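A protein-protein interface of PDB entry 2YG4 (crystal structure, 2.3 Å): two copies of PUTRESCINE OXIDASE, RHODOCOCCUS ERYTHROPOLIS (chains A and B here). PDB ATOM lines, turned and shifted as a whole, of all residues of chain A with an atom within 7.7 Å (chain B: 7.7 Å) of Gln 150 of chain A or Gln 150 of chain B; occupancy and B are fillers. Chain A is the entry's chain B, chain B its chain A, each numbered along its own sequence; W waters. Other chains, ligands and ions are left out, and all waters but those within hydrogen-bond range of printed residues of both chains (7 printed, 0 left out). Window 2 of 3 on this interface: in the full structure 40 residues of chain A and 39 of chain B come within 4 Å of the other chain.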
ATOM      1  N   THR A 145     -13.949 -15.821 -11.131  1.00  0.00           N
ATOM      2  CA  THR A 145     -14.687 -14.884 -11.915  1.00  0.00           C
ATOM      3  C   THR A 145     -14.942 -15.389 -13.304  1.00  0.00           C
ATOM      4  O   THR A 145     -15.355 -14.635 -14.171  1.00  0.00           O
ATOM      5  CB  THR A 145     -13.979 -13.541 -12.064  1.00  0.00           C
ATOM      6  OG1 THR A 145     -12.685 -13.780 -12.603  1.00  0.00           O
ATOM      7  CG2 THR A 145     -13.842 -12.762 -10.732  1.00  0.00           C
ATOM      8  N   VAL A 146     -14.657 -16.649 -13.557  1.00  0.00           N
ATOM      9  CA  VAL A 146     -14.951 -17.237 -14.880  1.00  0.00           C
ATOM     10  C   VAL A 146     -15.826 -18.444 -14.600  1.00  0.00           C
ATOM     11  O   VAL A 146     -15.541 -19.198 -13.636  1.00  0.00           O
ATOM     12  CB  VAL A 146     -13.636 -17.629 -15.612  1.00  0.00           C
ATOM     13  CG1 VAL A 146     -12.896 -18.702 -14.853  1.00  0.00           C
ATOM     14  CG2 VAL A 146     -13.890 -18.182 -16.950  1.00  0.00           C
ATOM     15  N   SER A 147     -16.881 -18.658 -15.379  1.00  0.00           N
ATOM     16  CA  SER A 147     -17.665 -19.899 -15.132  1.00  0.00           C
ATOM     17  C   SER A 147     -16.914 -21.164 -15.441  1.00  0.00           C
ATOM     18  O   SER A 147     -16.064 -21.165 -16.314  1.00  0.00           O
ATOM     19  CB  SER A 147     -18.988 -19.949 -15.918  1.00  0.00           C
ATOM     20  OG  SER A 147     -18.708 -19.924 -17.273  1.00  0.00           O
ATOM     21  N   PHE A 148     -17.283 -22.273 -14.799  1.00  0.00           N
ATOM     22  CA  PHE A 148     -16.703 -23.553 -15.182  1.00  0.00           C
ATOM     23  C   PHE A 148     -16.901 -23.829 -16.664  1.00  0.00           C
ATOM     24  O   PHE A 148     -16.016 -24.333 -17.290  1.00  0.00           O
ATOM     25  CB  PHE A 148     -17.320 -24.715 -14.384  1.00  0.00           C
ATOM     26  CG  PHE A 148     -16.455 -25.948 -14.381  1.00  0.00           C
ATOM     27  CD1 PHE A 148     -15.042 -25.837 -14.344  1.00  0.00           C
ATOM     28  CD2 PHE A 148     -17.017 -27.215 -14.482  1.00  0.00           C
ATOM     29  CE1 PHE A 148     -14.219 -27.009 -14.334  1.00  0.00           C
ATOM     30  CE2 PHE A 148     -16.227 -28.352 -14.471  1.00  0.00           C
ATOM     31  CZ  PHE A 148     -14.800 -28.241 -14.369  1.00  0.00           C
ATOM     32  N   LYS A 149     -18.046 -23.486 -17.244  1.00  0.00           N
ATOM     33  CA  LYS A 149     -18.278 -23.741 -18.683  1.00  0.00           C
ATOM     34  C   LYS A 149     -17.253 -22.995 -19.511  1.00  0.00           C
ATOM     35  O   LYS A 149     -16.755 -23.535 -20.523  1.00  0.00           O
ATOM     36  CB  LYS A 149     -19.659 -23.223 -19.092  1.00  0.00           C
ATOM     37  CG  LYS A 149     -19.877 -23.066 -20.577  1.00  0.00           C
ATOM     38  CD  LYS A 149     -21.376 -22.883 -20.950  1.00  0.00           C
ATOM     39  CE  LYS A 149     -21.494 -22.739 -22.509  1.00  0.00           C
ATOM     40  NZ  LYS A 149     -22.745 -22.094 -22.930  1.00  0.00           N
ATOM     41  N   GLN A 150     -17.010 -21.718 -19.137  1.00  0.00           N
ATOM     42  CA  GLN A 150     -16.132 -20.846 -19.922  1.00  0.00           C
ATOM     43  C   GLN A 150     -14.649 -21.269 -19.717  1.00  0.00           C
ATOM     44  O   GLN A 150     -13.854 -21.226 -20.646  1.00  0.00           O
ATOM     45  CB  GLN A 150     -16.311 -19.369 -19.542  1.00  0.00           C
ATOM     46  CG  GLN A 150     -15.393 -18.442 -20.325  1.00  0.00           C
ATOM     47  CD  GLN A 150     -15.731 -18.348 -21.846  1.00  0.00           C
ATOM     48  OE1 GLN A 150     -16.874 -18.029 -22.259  1.00  0.00           O
ATOM     49  NE2 GLN A 150     -14.716 -18.596 -22.679  1.00  0.00           N
ATOM     50  N   TRP A 151     -14.292 -21.661 -18.497  1.00  0.00           N
ATOM     51  CA  TRP A 151     -12.965 -22.124 -18.223  1.00  0.00           C
ATOM     52  C   TRP A 151     -12.689 -23.394 -19.036  1.00  0.00           C
ATOM     53  O   TRP A 151     -11.610 -23.533 -19.582  1.00  0.00           O
ATOM     54  CB  TRP A 151     -12.835 -22.428 -16.742  1.00  0.00           C
ATOM     55  CG  TRP A 151     -11.473 -22.830 -16.306  1.00  0.00           C
ATOM     56  CD1 TRP A 151     -10.413 -21.981 -15.908  1.00  0.00           C
ATOM     57  CD2 TRP A 151     -10.970 -24.165 -16.186  1.00  0.00           C
ATOM     58  NE1 TRP A 151      -9.305 -22.748 -15.583  1.00  0.00           N
ATOM     59  CE2 TRP A 151      -9.615 -24.074 -15.733  1.00  0.00           C
ATOM     60  CE3 TRP A 151     -11.511 -25.425 -16.449  1.00  0.00           C
ATOM     61  CZ2 TRP A 151      -8.821 -25.208 -15.514  1.00  0.00           C
ATOM     62  CZ3 TRP A 151     -10.738 -26.561 -16.198  1.00  0.00           C
ATOM     63  CH2 TRP A 151      -9.396 -26.451 -15.745  1.00  0.00           C
ATOM     64  N   LEU A 152     -13.649 -24.315 -19.140  1.00  0.00           N
ATOM     65  CA  LEU A 152     -13.391 -25.513 -19.952  1.00  0.00           C
ATOM     66  C   LEU A 152     -13.184 -25.154 -21.429  1.00  0.00           C
ATOM     67  O   LEU A 152     -12.300 -25.691 -22.056  1.00  0.00           O
ATOM     68  CB  LEU A 152     -14.489 -26.524 -19.839  1.00  0.00           C
ATOM     69  CG  LEU A 152     -14.572 -27.187 -18.463  1.00  0.00           C
ATOM     70  CD1 LEU A 152     -15.926 -27.928 -18.350  1.00  0.00           C
ATOM     71  CD2 LEU A 152     -13.429 -28.154 -18.272  1.00  0.00           C
ATOM     72  N   ILE A 153     -14.000 -24.256 -21.970  1.00  0.00           N
ATOM     73  CA  ILE A 153     -13.792 -23.722 -23.313  1.00  0.00           C
ATOM     74  C   ILE A 153     -12.384 -23.115 -23.479  1.00  0.00           C
ATOM     75  O   ILE A 153     -11.753 -23.363 -24.477  1.00  0.00           O
ATOM     76  CB  ILE A 153     -14.867 -22.663 -23.677  1.00  0.00           C
ATOM     77  CG1 ILE A 153     -16.231 -23.363 -23.918  1.00  0.00           C
ATOM     78  CG2 ILE A 153     -14.363 -21.820 -24.896  1.00  0.00           C
ATOM     79  CD1 ILE A 153     -17.434 -22.368 -24.020  1.00  0.00           C
ATOM     80  N   ASN A 154     -11.893 -22.342 -22.508  1.00  0.00           N
ATOM     81  CA  ASN A 154     -10.532 -21.787 -22.539  1.00  0.00           C
ATOM     82  C   ASN A 154      -9.444 -22.860 -22.481  1.00  0.00           C
ATOM     83  O   ASN A 154      -8.315 -22.614 -22.844  1.00  0.00           O
ATOM     84  CB  ASN A 154     -10.302 -20.821 -21.346  1.00  0.00           C
ATOM     85  CG  ASN A 154     -11.136 -19.529 -21.463  1.00  0.00           C
ATOM     86  OD1 ASN A 154     -11.699 -19.197 -22.543  1.00  0.00           O
ATOM     87  ND2 ASN A 154     -11.213 -18.782 -20.346  1.00  0.00           N
ATOM     88  N   GLN A 155      -9.753 -24.040 -21.975  1.00  0.00           N
ATOM     89  CA  GLN A 155      -8.744 -25.095 -21.875  1.00  0.00           C
ATOM     90  C   GLN A 155      -8.794 -26.062 -23.048  1.00  0.00           C
ATOM     91  O   GLN A 155      -7.780 -26.580 -23.458  1.00  0.00           O
ATOM     92  CB  GLN A 155      -8.901 -25.929 -20.596  1.00  0.00           C
ATOM     93  CG  GLN A 155      -8.922 -25.149 -19.325  1.00  0.00           C
ATOM     94  CD  GLN A 155      -7.785 -24.163 -19.204  1.00  0.00           C
ATOM     95  OE1 GLN A 155      -7.992 -22.974 -18.896  1.00  0.00           O
ATOM     96  NE2 GLN A 155      -6.581 -24.652 -19.387  1.00  0.00           N
ATOM     97  N   SER A 156      -9.961 -26.327 -23.607  1.00  0.00           N
ATOM     98  CA  SER A 156      -9.993 -27.353 -24.609  1.00  0.00           C
ATOM     99  C   SER A 156     -10.976 -27.085 -25.742  1.00  0.00           C
ATOM    100  O   SER A 156     -12.082 -26.583 -25.504  1.00  0.00           O
ATOM    101  CB  SER A 156     -10.379 -28.645 -23.937  1.00  0.00           C
ATOM    102  OG  SER A 156     -10.575 -29.658 -24.904  1.00  0.00           O
ATOM    103  N   ARG A 162     -15.149 -31.722 -22.773  1.00  0.00           N
ATOM    104  CA  ARG A 162     -15.629 -30.654 -21.847  1.00  0.00           C
ATOM    105  C   ARG A 162     -16.950 -31.086 -21.228  1.00  0.00           C
ATOM    106  O   ARG A 162     -17.193 -30.880 -20.017  1.00  0.00           O
ATOM    107  CB  ARG A 162     -15.839 -29.282 -22.552  1.00  0.00           C
ATOM    108  CG  ARG A 162     -14.606 -28.699 -23.135  1.00  0.00           C
ATOM    109  CD  ARG A 162     -14.844 -27.291 -23.688  1.00  0.00           C
ATOM    110  NE  ARG A 162     -15.942 -27.276 -24.634  1.00  0.00           N
ATOM    111  CZ  ARG A 162     -15.807 -26.904 -25.904  1.00  0.00           C
ATOM    112  NH1 ARG A 162     -14.612 -26.536 -26.342  1.00  0.00           N
ATOM    113  NH2 ARG A 162     -16.866 -26.835 -26.714  1.00  0.00           N
ATOM    114  N   ALA A 178     -23.123 -25.848 -15.689  1.00  0.00           N
ATOM    115  CA  ALA A 178     -21.724 -25.416 -15.614  1.00  0.00           C
ATOM    116  C   ALA A 178     -21.546 -23.927 -15.872  1.00  0.00           C
ATOM    117  O   ALA A 178     -20.475 -23.349 -15.561  1.00  0.00           O
ATOM    118  CB  ALA A 178     -20.910 -26.190 -16.617  1.00  0.00           C
ATOM    119  N   HIS A 179     -22.516 -23.301 -16.523  1.00  0.00           N
ATOM    120  CA  HIS A 179     -22.388 -21.861 -16.773  1.00  0.00           C
ATOM    121  C   HIS A 179     -22.703 -21.051 -15.501  1.00  0.00           C
ATOM    122  O   HIS A 179     -22.590 -19.841 -15.495  1.00  0.00           O
ATOM    123  CB  HIS A 179     -23.309 -21.414 -17.918  1.00  0.00           C
ATOM    124  CG  HIS A 179     -24.756 -21.806 -17.739  1.00  0.00           C
ATOM    125  ND1 HIS A 179     -25.676 -21.008 -17.081  1.00  0.00           N
ATOM    126  CD2 HIS A 179     -25.459 -22.869 -18.195  1.00  0.00           C
ATOM    127  CE1 HIS A 179     -26.873 -21.580 -17.098  1.00  0.00           C
ATOM    128  NE2 HIS A 179     -26.774 -22.689 -17.797  1.00  0.00           N
ATOM    129  N   PHE A 181     -21.724 -21.684 -12.033  1.00  0.00           N
ATOM    130  CA  PHE A 181     -20.764 -21.634 -10.930  1.00  0.00           C
ATOM    131  C   PHE A 181     -19.350 -21.523 -11.506  1.00  0.00           C
ATOM    132  O   PHE A 181     -19.118 -21.781 -12.702  1.00  0.00           O
ATOM    133  CB  PHE A 181     -20.842 -22.899 -10.001  1.00  0.00           C
ATOM    134  CG  PHE A 181     -20.618 -24.199 -10.728  1.00  0.00           C
ATOM    135  CD1 PHE A 181     -19.339 -24.703 -10.900  1.00  0.00           C
ATOM    136  CD2 PHE A 181     -21.701 -24.893 -11.289  1.00  0.00           C
ATOM    137  CE1 PHE A 181     -19.138 -25.921 -11.569  1.00  0.00           C
ATOM    138  CE2 PHE A 181     -21.522 -26.133 -12.011  1.00  0.00           C
ATOM    139  CZ  PHE A 181     -20.227 -26.629 -12.152  1.00  0.00           C
ATOM    140  N   ALA A 183     -15.023 -21.795 -12.134  1.00  0.00           N
ATOM    141  CA  ALA A 183     -13.879 -22.702 -12.055  1.00  0.00           C
ATOM    142  C   ALA A 183     -13.397 -22.952 -10.595  1.00  0.00           C
ATOM    143  O   ALA A 183     -13.136 -24.128 -10.210  1.00  0.00           O
ATOM    144  CB  ALA A 183     -12.740 -22.239 -12.964  1.00  0.00           C
ATOM    145  N   LEU A 401     -22.120 -17.488  -8.915  1.00  0.00           N
ATOM    146  CA  LEU A 401     -20.840 -17.266  -9.567  1.00  0.00           C
ATOM    147  C   LEU A 401     -20.231 -15.985  -9.039  1.00  0.00           C
ATOM    148  O   LEU A 401     -20.810 -14.887  -9.134  1.00  0.00           O
ATOM    149  CB  LEU A 401     -20.942 -17.215 -11.102  1.00  0.00           C
ATOM    150  CG  LEU A 401     -19.661 -17.479 -11.870  1.00  0.00           C
ATOM    151  CD1 LEU A 401     -19.995 -17.683 -13.288  1.00  0.00           C
ATOM    152  CD2 LEU A 401     -18.646 -16.259 -11.737  1.00  0.00           C
ATOM    153  N   THR B 145     -26.197 -17.456 -20.633  1.00  0.00           N
ATOM    154  CA  THR B 145     -25.187 -18.348 -20.106  1.00  0.00           C
ATOM    155  C   THR B 145     -23.743 -17.808 -20.216  1.00  0.00           C
ATOM    156  O   THR B 145     -22.785 -18.538 -19.977  1.00  0.00           O
ATOM    157  CB  THR B 145     -25.235 -19.743 -20.814  1.00  0.00           C
ATOM    158  OG1 THR B 145     -24.985 -19.529 -22.195  1.00  0.00           O
ATOM    159  CG2 THR B 145     -26.568 -20.381 -20.641  1.00  0.00           C
ATOM    160  N   VAL B 146     -23.580 -16.556 -20.602  1.00  0.00           N
ATOM    161  CA  VAL B 146     -22.278 -15.960 -20.669  1.00  0.00           C
ATOM    162  C   VAL B 146     -22.391 -14.786 -19.679  1.00  0.00           C
ATOM    163  O   VAL B 146     -23.432 -14.090 -19.651  1.00  0.00           O
ATOM    164  CB  VAL B 146     -21.951 -15.508 -22.135  1.00  0.00           C
ATOM    165  CG1 VAL B 146     -23.006 -14.502 -22.718  1.00  0.00           C
ATOM    166  CG2 VAL B 146     -20.611 -14.845 -22.207  1.00  0.00           C
ATOM    167  N   SER B 147     -21.388 -14.566 -18.824  1.00  0.00           N
ATOM    168  CA  SER B 147     -21.468 -13.387 -17.924  1.00  0.00           C
ATOM    169  C   SER B 147     -21.373 -12.071 -18.716  1.00  0.00           C
ATOM    170  O   SER B 147     -20.843 -12.069 -19.796  1.00  0.00           O
ATOM    171  CB  SER B 147     -20.357 -13.405 -16.883  1.00  0.00           C
ATOM    172  OG  SER B 147     -19.100 -13.196 -17.540  1.00  0.00           O
ATOM    173  N   PHE B 148     -21.861 -10.962 -18.160  1.00  0.00           N
ATOM    174  CA  PHE B 148     -21.735  -9.698 -18.863  1.00  0.00           C
ATOM    175  C   PHE B 148     -20.257  -9.326 -19.073  1.00  0.00           C
ATOM    176  O   PHE B 148     -19.876  -8.767 -20.154  1.00  0.00           O
ATOM    177  CB  PHE B 148     -22.502  -8.580 -18.157  1.00  0.00           C
ATOM    178  CG  PHE B 148     -22.628  -7.317 -18.957  1.00  0.00           C
ATOM    179  CD1 PHE B 148     -23.082  -7.354 -20.246  1.00  0.00           C
ATOM    180  CD2 PHE B 148     -22.341  -6.054 -18.373  1.00  0.00           C
ATOM    181  CE1 PHE B 148     -23.228  -6.162 -20.970  1.00  0.00           C
ATOM    182  CE2 PHE B 148     -22.476  -4.875 -19.096  1.00  0.00           C
ATOM    183  CZ  PHE B 148     -22.916  -4.930 -20.381  1.00  0.00           C
ATOM    184  N   LYS B 149     -19.418  -9.658 -18.103  1.00  0.00           N
ATOM    185  CA  LYS B 149     -18.022  -9.351 -18.277  1.00  0.00           C
ATOM    186  C   LYS B 149     -17.456 -10.171 -19.477  1.00  0.00           C
ATOM    187  O   LYS B 149     -16.714  -9.642 -20.285  1.00  0.00           O
ATOM    188  CB  LYS B 149     -17.237  -9.664 -17.005  1.00  0.00           C
ATOM    189  CG  LYS B 149     -15.701  -9.654 -17.220  1.00  0.00           C
ATOM    190  CD  LYS B 149     -14.963 -10.516 -16.193  1.00  0.00           C
ATOM    191  CE  LYS B 149     -13.732  -9.733 -15.663  1.00  0.00           C
ATOM    192  NZ  LYS B 149     -12.758 -10.725 -15.126  1.00  0.00           N
ATOM    193  N   GLN B 150     -17.787 -11.457 -19.586  1.00  0.00           N
ATOM    194  CA  GLN B 150     -17.215 -12.243 -20.650  1.00  0.00           C
ATOM    195  C   GLN B 150     -17.794 -11.752 -22.009  1.00  0.00           C
ATOM    196  O   GLN B 150     -17.071 -11.647 -23.033  1.00  0.00           O
ATOM    197  CB  GLN B 150     -17.513 -13.731 -20.453  1.00  0.00           C
ATOM    198  CG  GLN B 150     -17.027 -14.578 -21.617  1.00  0.00           C
ATOM    199  CD  GLN B 150     -15.506 -14.655 -21.635  1.00  0.00           C
ATOM    200  OE1 GLN B 150     -14.870 -14.946 -20.618  1.00  0.00           O
ATOM    201  NE2 GLN B 150     -14.909 -14.359 -22.789  1.00  0.00           N
ATOM    202  N   TRP B 151     -19.070 -11.394 -21.997  1.00  0.00           N
ATOM    203  CA  TRP B 151     -19.681 -10.806 -23.200  1.00  0.00           C
ATOM    204  C   TRP B 151     -18.971  -9.527 -23.613  1.00  0.00           C
ATOM    205  O   TRP B 151     -18.737  -9.334 -24.769  1.00  0.00           O
ATOM    206  CB  TRP B 151     -21.150 -10.513 -22.967  1.00  0.00           C
ATOM    207  CG  TRP B 151     -21.903 -10.047 -24.197  1.00  0.00           C
ATOM    208  CD1 TRP B 151     -22.577 -10.863 -25.126  1.00  0.00           C
ATOM    209  CD2 TRP B 151     -22.129  -8.688 -24.627  1.00  0.00           C
ATOM    210  NE1 TRP B 151     -23.187 -10.069 -26.082  1.00  0.00           N
ATOM    211  CE2 TRP B 151     -22.919  -8.747 -25.820  1.00  0.00           C
ATOM    212  CE3 TRP B 151     -21.769  -7.437 -24.117  1.00  0.00           C
ATOM    213  CZ2 TRP B 151     -23.318  -7.603 -26.518  1.00  0.00           C
ATOM    214  CZ3 TRP B 151     -22.159  -6.283 -24.829  1.00  0.00           C
ATOM    215  CH2 TRP B 151     -22.938  -6.390 -26.018  1.00  0.00           C
ATOM    216  N   LEU B 152     -18.595  -8.659 -22.670  1.00  0.00           N
ATOM    217  CA  LEU B 152     -17.887  -7.432 -23.033  1.00  0.00           C
ATOM    218  C   LEU B 152     -16.535  -7.764 -23.649  1.00  0.00           C
ATOM    219  O   LEU B 152     -16.174  -7.195 -24.697  1.00  0.00           O
ATOM    220  CB  LEU B 152     -17.707  -6.490 -21.839  1.00  0.00           C
ATOM    221  CG  LEU B 152     -18.983  -5.757 -21.380  1.00  0.00           C
ATOM    222  CD1 LEU B 152     -18.796  -5.164 -20.003  1.00  0.00           C
ATOM    223  CD2 LEU B 152     -19.447  -4.687 -22.430  1.00  0.00           C
ATOM    224  N   ILE B 153     -15.818  -8.707 -23.025  1.00  0.00           N
ATOM    225  CA  ILE B 153     -14.525  -9.189 -23.551  1.00  0.00           C
ATOM    226  C   ILE B 153     -14.706  -9.722 -24.984  1.00  0.00           C
ATOM    227  O   ILE B 153     -13.909  -9.400 -25.841  1.00  0.00           O
ATOM    228  CB  ILE B 153     -13.900 -10.257 -22.659  1.00  0.00           C
ATOM    229  CG1 ILE B 153     -13.447  -9.635 -21.308  1.00  0.00           C
ATOM    230  CG2 ILE B 153     -12.775 -11.019 -23.397  1.00  0.00           C
ATOM    231  CD1 ILE B 153     -13.220 -10.709 -20.250  1.00  0.00           C
ATOM    232  N   ASN B 154     -15.780 -10.473 -25.255  1.00  0.00           N
ATOM    233  CA  ASN B 154     -16.036 -10.934 -26.618  1.00  0.00           C
ATOM    234  C   ASN B 154     -16.323  -9.830 -27.619  1.00  0.00           C
ATOM    235  O   ASN B 154     -16.135 -10.001 -28.816  1.00  0.00           O
ATOM    236  CB  ASN B 154     -17.223 -11.919 -26.644  1.00  0.00           C
ATOM    237  CG  ASN B 154     -16.921 -13.194 -25.921  1.00  0.00           C
ATOM    238  OD1 ASN B 154     -15.757 -13.513 -25.688  1.00  0.00           O
ATOM    239  ND2 ASN B 154     -17.954 -13.921 -25.530  1.00  0.00           N
ATOM    240  N   GLN B 155     -16.863  -8.721 -27.153  1.00  0.00           N
ATOM    241  CA  GLN B 155     -17.297  -7.663 -28.058  1.00  0.00           C
ATOM    242  C   GLN B 155     -16.141  -6.712 -28.315  1.00  0.00           C
ATOM    243  O   GLN B 155     -16.060  -6.189 -29.408  1.00  0.00           O
ATOM    244  CB  GLN B 155     -18.458  -6.832 -27.496  1.00  0.00           C
ATOM    245  CG  GLN B 155     -19.817  -7.584 -27.259  1.00  0.00           C
ATOM    246  CD  GLN B 155     -20.163  -8.606 -28.382  1.00  0.00           C
ATOM    247  OE1 GLN B 155     -20.129  -9.827 -28.145  1.00  0.00           O
ATOM    248  NE2 GLN B 155     -20.500  -8.115 -29.570  1.00  0.00           N
ATOM    249  N   SER B 156     -15.247  -6.493 -27.343  1.00  0.00           N
ATOM    250  CA  SER B 156     -14.290  -5.387 -27.488  1.00  0.00           C
ATOM    251  C   SER B 156     -13.043  -5.702 -26.726  1.00  0.00           C
ATOM    252  O   SER B 156     -13.149  -6.245 -25.635  1.00  0.00           O
ATOM    253  CB  SER B 156     -14.872  -4.055 -26.976  1.00  0.00           C
ATOM    254  OG  SER B 156     -13.823  -3.054 -26.977  1.00  0.00           O
ATOM    255  N   ARG B 162     -14.875  -1.013 -22.019  1.00  0.00           N
ATOM    256  CA  ARG B 162     -15.617  -2.047 -21.307  1.00  0.00           C
ATOM    257  C   ARG B 162     -15.953  -1.635 -19.878  1.00  0.00           C
ATOM    258  O   ARG B 162     -17.104  -1.723 -19.442  1.00  0.00           O
ATOM    259  CB  ARG B 162     -14.837  -3.394 -21.286  1.00  0.00           C
ATOM    260  CG  ARG B 162     -14.608  -4.024 -22.671  1.00  0.00           C
ATOM    261  CD  ARG B 162     -14.082  -5.476 -22.587  1.00  0.00           C
ATOM    262  NE  ARG B 162     -12.916  -5.631 -21.733  1.00  0.00           N
ATOM    263  CZ  ARG B 162     -11.774  -6.243 -22.071  1.00  0.00           C
ATOM    264  NH1 ARG B 162     -11.591  -6.843 -23.278  1.00  0.00           N
ATOM    265  NH2 ARG B 162     -10.816  -6.326 -21.147  1.00  0.00           N
ATOM    266  N   ALA B 178     -19.780  -7.324 -12.814  1.00  0.00           N
ATOM    267  CA  ALA B 178     -20.166  -7.808 -14.161  1.00  0.00           C
ATOM    268  C   ALA B 178     -19.879  -9.311 -14.405  1.00  0.00           C
ATOM    269  O   ALA B 178     -20.504  -9.925 -15.294  1.00  0.00           O
ATOM    270  CB  ALA B 178     -19.502  -6.909 -15.320  1.00  0.00           C
ATOM    271  N   HIS B 179     -18.972  -9.928 -13.619  1.00  0.00           N
ATOM    272  CA  HIS B 179     -18.732 -11.377 -13.794  1.00  0.00           C
ATOM    273  C   HIS B 179     -19.831 -12.188 -13.155  1.00  0.00           C
ATOM    274  O   HIS B 179     -19.876 -13.370 -13.354  1.00  0.00           O
ATOM    275  CB  HIS B 179     -17.394 -11.810 -13.213  1.00  0.00           C
ATOM    276  CG  HIS B 179     -17.228 -11.485 -11.762  1.00  0.00           C
ATOM    277  ND1 HIS B 179     -17.660 -12.336 -10.758  1.00  0.00           N
ATOM    278  CD2 HIS B 179     -16.645 -10.433 -11.133  1.00  0.00           C
ATOM    279  CE1 HIS B 179     -17.392 -11.800  -9.576  1.00  0.00           C
ATOM    280  NE2 HIS B 179     -16.753 -10.667  -9.776  1.00  0.00           N
ATOM    281  N   PHE B 181     -23.401 -11.606 -13.291  1.00  0.00           N
ATOM    282  CA  PHE B 181     -24.735 -11.608 -13.874  1.00  0.00           C
ATOM    283  C   PHE B 181     -24.589 -11.777 -15.414  1.00  0.00           C
ATOM    284  O   PHE B 181     -23.506 -11.553 -15.947  1.00  0.00           O
ATOM    285  CB  PHE B 181     -25.543 -10.342 -13.483  1.00  0.00           C
ATOM    286  CG  PHE B 181     -24.932  -9.032 -13.961  1.00  0.00           C
ATOM    287  CD1 PHE B 181     -25.074  -8.607 -15.284  1.00  0.00           C
ATOM    288  CD2 PHE B 181     -24.238  -8.203 -13.078  1.00  0.00           C
ATOM    289  CE1 PHE B 181     -24.549  -7.364 -15.725  1.00  0.00           C
ATOM    290  CE2 PHE B 181     -23.710  -6.940 -13.490  1.00  0.00           C
ATOM    291  CZ  PHE B 181     -23.860  -6.531 -14.818  1.00  0.00           C
ATOM    292  N   ALA B 183     -25.082 -11.538 -19.712  1.00  0.00           N
ATOM    293  CA  ALA B 183     -25.432 -10.513 -20.752  1.00  0.00           C
ATOM    294  C   ALA B 183     -26.936 -10.280 -20.889  1.00  0.00           C
ATOM    295  O   ALA B 183     -27.404  -9.107 -21.045  1.00  0.00           O
ATOM    296  CB  ALA B 183     -24.797 -10.887 -22.106  1.00  0.00           C
ATOM    297  N   LEU B 401     -26.344 -15.962 -12.124  1.00  0.00           N
ATOM    298  CA  LEU B 401     -26.078 -16.083 -13.512  1.00  0.00           C
ATOM    299  C   LEU B 401     -26.747 -17.368 -13.994  1.00  0.00           C
ATOM    300  O   LEU B 401     -26.539 -18.427 -13.466  1.00  0.00           O
ATOM    301  CB  LEU B 401     -24.563 -16.100 -13.720  1.00  0.00           C
ATOM    302  CG  LEU B 401     -24.184 -15.779 -15.165  1.00  0.00           C
ATOM    303  CD1 LEU B 401     -22.739 -15.398 -15.188  1.00  0.00           C
ATOM    304  CD2 LEU B 401     -24.406 -16.918 -16.096  1.00  0.00           C
HETATM  305  O   HOH W   1     -18.013 -14.692 -15.269  1.00  0.00           O
HETATM  306  O   HOH W   2     -24.235 -14.968  -9.838  1.00  0.00           O
HETATM  307  O   HOH W   3     -17.693 -16.892 -24.597  1.00  0.00           O
HETATM  308  O   HOH W   4     -21.941 -19.280 -22.558  1.00  0.00           O
HETATM  309  O   HOH W   5     -10.659 -11.862 -12.650  1.00  0.00           O
HETATM  310  O   HOH W   6     -12.175 -15.919 -20.462  1.00  0.00           O
HETATM  311  O   HOH W   7     -25.050 -18.273 -10.475  1.00  0.00           O
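The side-chain hydroxyl of Thr 145 of chain B is in hydrogen-bond range of the side-chain amino group of Lys 149 of chain A.
Thr 145 of chain A touches Lys 149 of chain B, and with the chains exchanged Lys 149 of chain A touches Thr 145 of chain B. Thr 145 of chain A touches His 179 of chain B, and with the chains exchanged His 179 of chain A touches Thr 145 of chain B. Gln 150 of chain B touches its own counterpart, Gln 150 of chain A. His 179 of chain A touches Leu 401 of chain B, and with the chains exchanged Leu 401 of chain A touches His 179 of chain B.
Among the printed residues, pairs that only touch across the chains: His 179 of chain A with Leu 401 of chain B (3.5 Å), Gln 150 of chain A with Gln 150 of chain B (3.5 Å), Leu 401 of chain A with His 179 of chain B (3.5 Å), His 179 of chain A with Thr 145 of chain B (3.6 Å), Thr 145 of chain A with His 179 of chain B (3.6 Å) and Thr 145 of chain A with Lys 149 of chain B (3.96 Å).
Of the printed residues of chain B, Gln 150 of chain A touches Gln 150. Gln 150 of chain B touches just one residue of chain A: Gln 150 (3.5 Å). Printed residues of chain A within 4 Å of Thr 145 of chain B: Lys 149 (3.5 Å) and His 179 (3.6 Å). Of the printed residues of chain A, His 179 of chain B touches Thr 145 and Leu 401. Ala 183 of chain A touches none of the printed residues of chain B. Arg 162 of chain A touches none of the printed residues of chain B. The nearest residue of chain A that does not touch Gln 150 of chain B is Val 146 of chain A (5.0 Å).
Water W3 bridges the side-chain amide oxygen of Gln 150 of chain A (2.7 Å) and the side-chain amide nitrogen of Asn 154 of chain B (3.1 Å). Water W1 lies within hydrogen-bond range of the backbone carbonyl oxygen of Thr 145 of chain A, the side-chain hydroxyl of Ser 147 of chain B and the backbone carbonyl oxygen of His 179 of chain B. Water W2 lies within hydrogen-bond range of the backbone NH (N) of Leu 401 of chain B (3.3 Å) and the backbone NH (N) of Leu 401 of chain A (3.4 Å).
Hydrophobic or aromatic side chains of chain A within 4 Å of the printed part of chain B: His 179 and Leu 401. Of the 18 printed residues of chain B, 5 touch a printed residue of chain A. Among the printed residues, 7 pairs touch across the chains. Among the printed residues, no Asp or Glu carboxylate lies within 4 Å of a Lys or Arg side-chain nitrogen of the other chain.
The side-chain amide nitrogen (NE2) of Gln 150 of chain B lies within hydrogen-bond range of the side-chain amide oxygen (OD1) of Asn 154 of chain B (3.1 Å). The side-chain amide nitrogen of Gln 150 of chain A lies within hydrogen-bond range of the side-chain amide oxygen of Asn 154 of chain A. The side-chain hydroxyl (OG) of Ser 147 of chain A sits at hydrogen-bond distance from the backbone NH (N) of Gln 150 of chain A.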
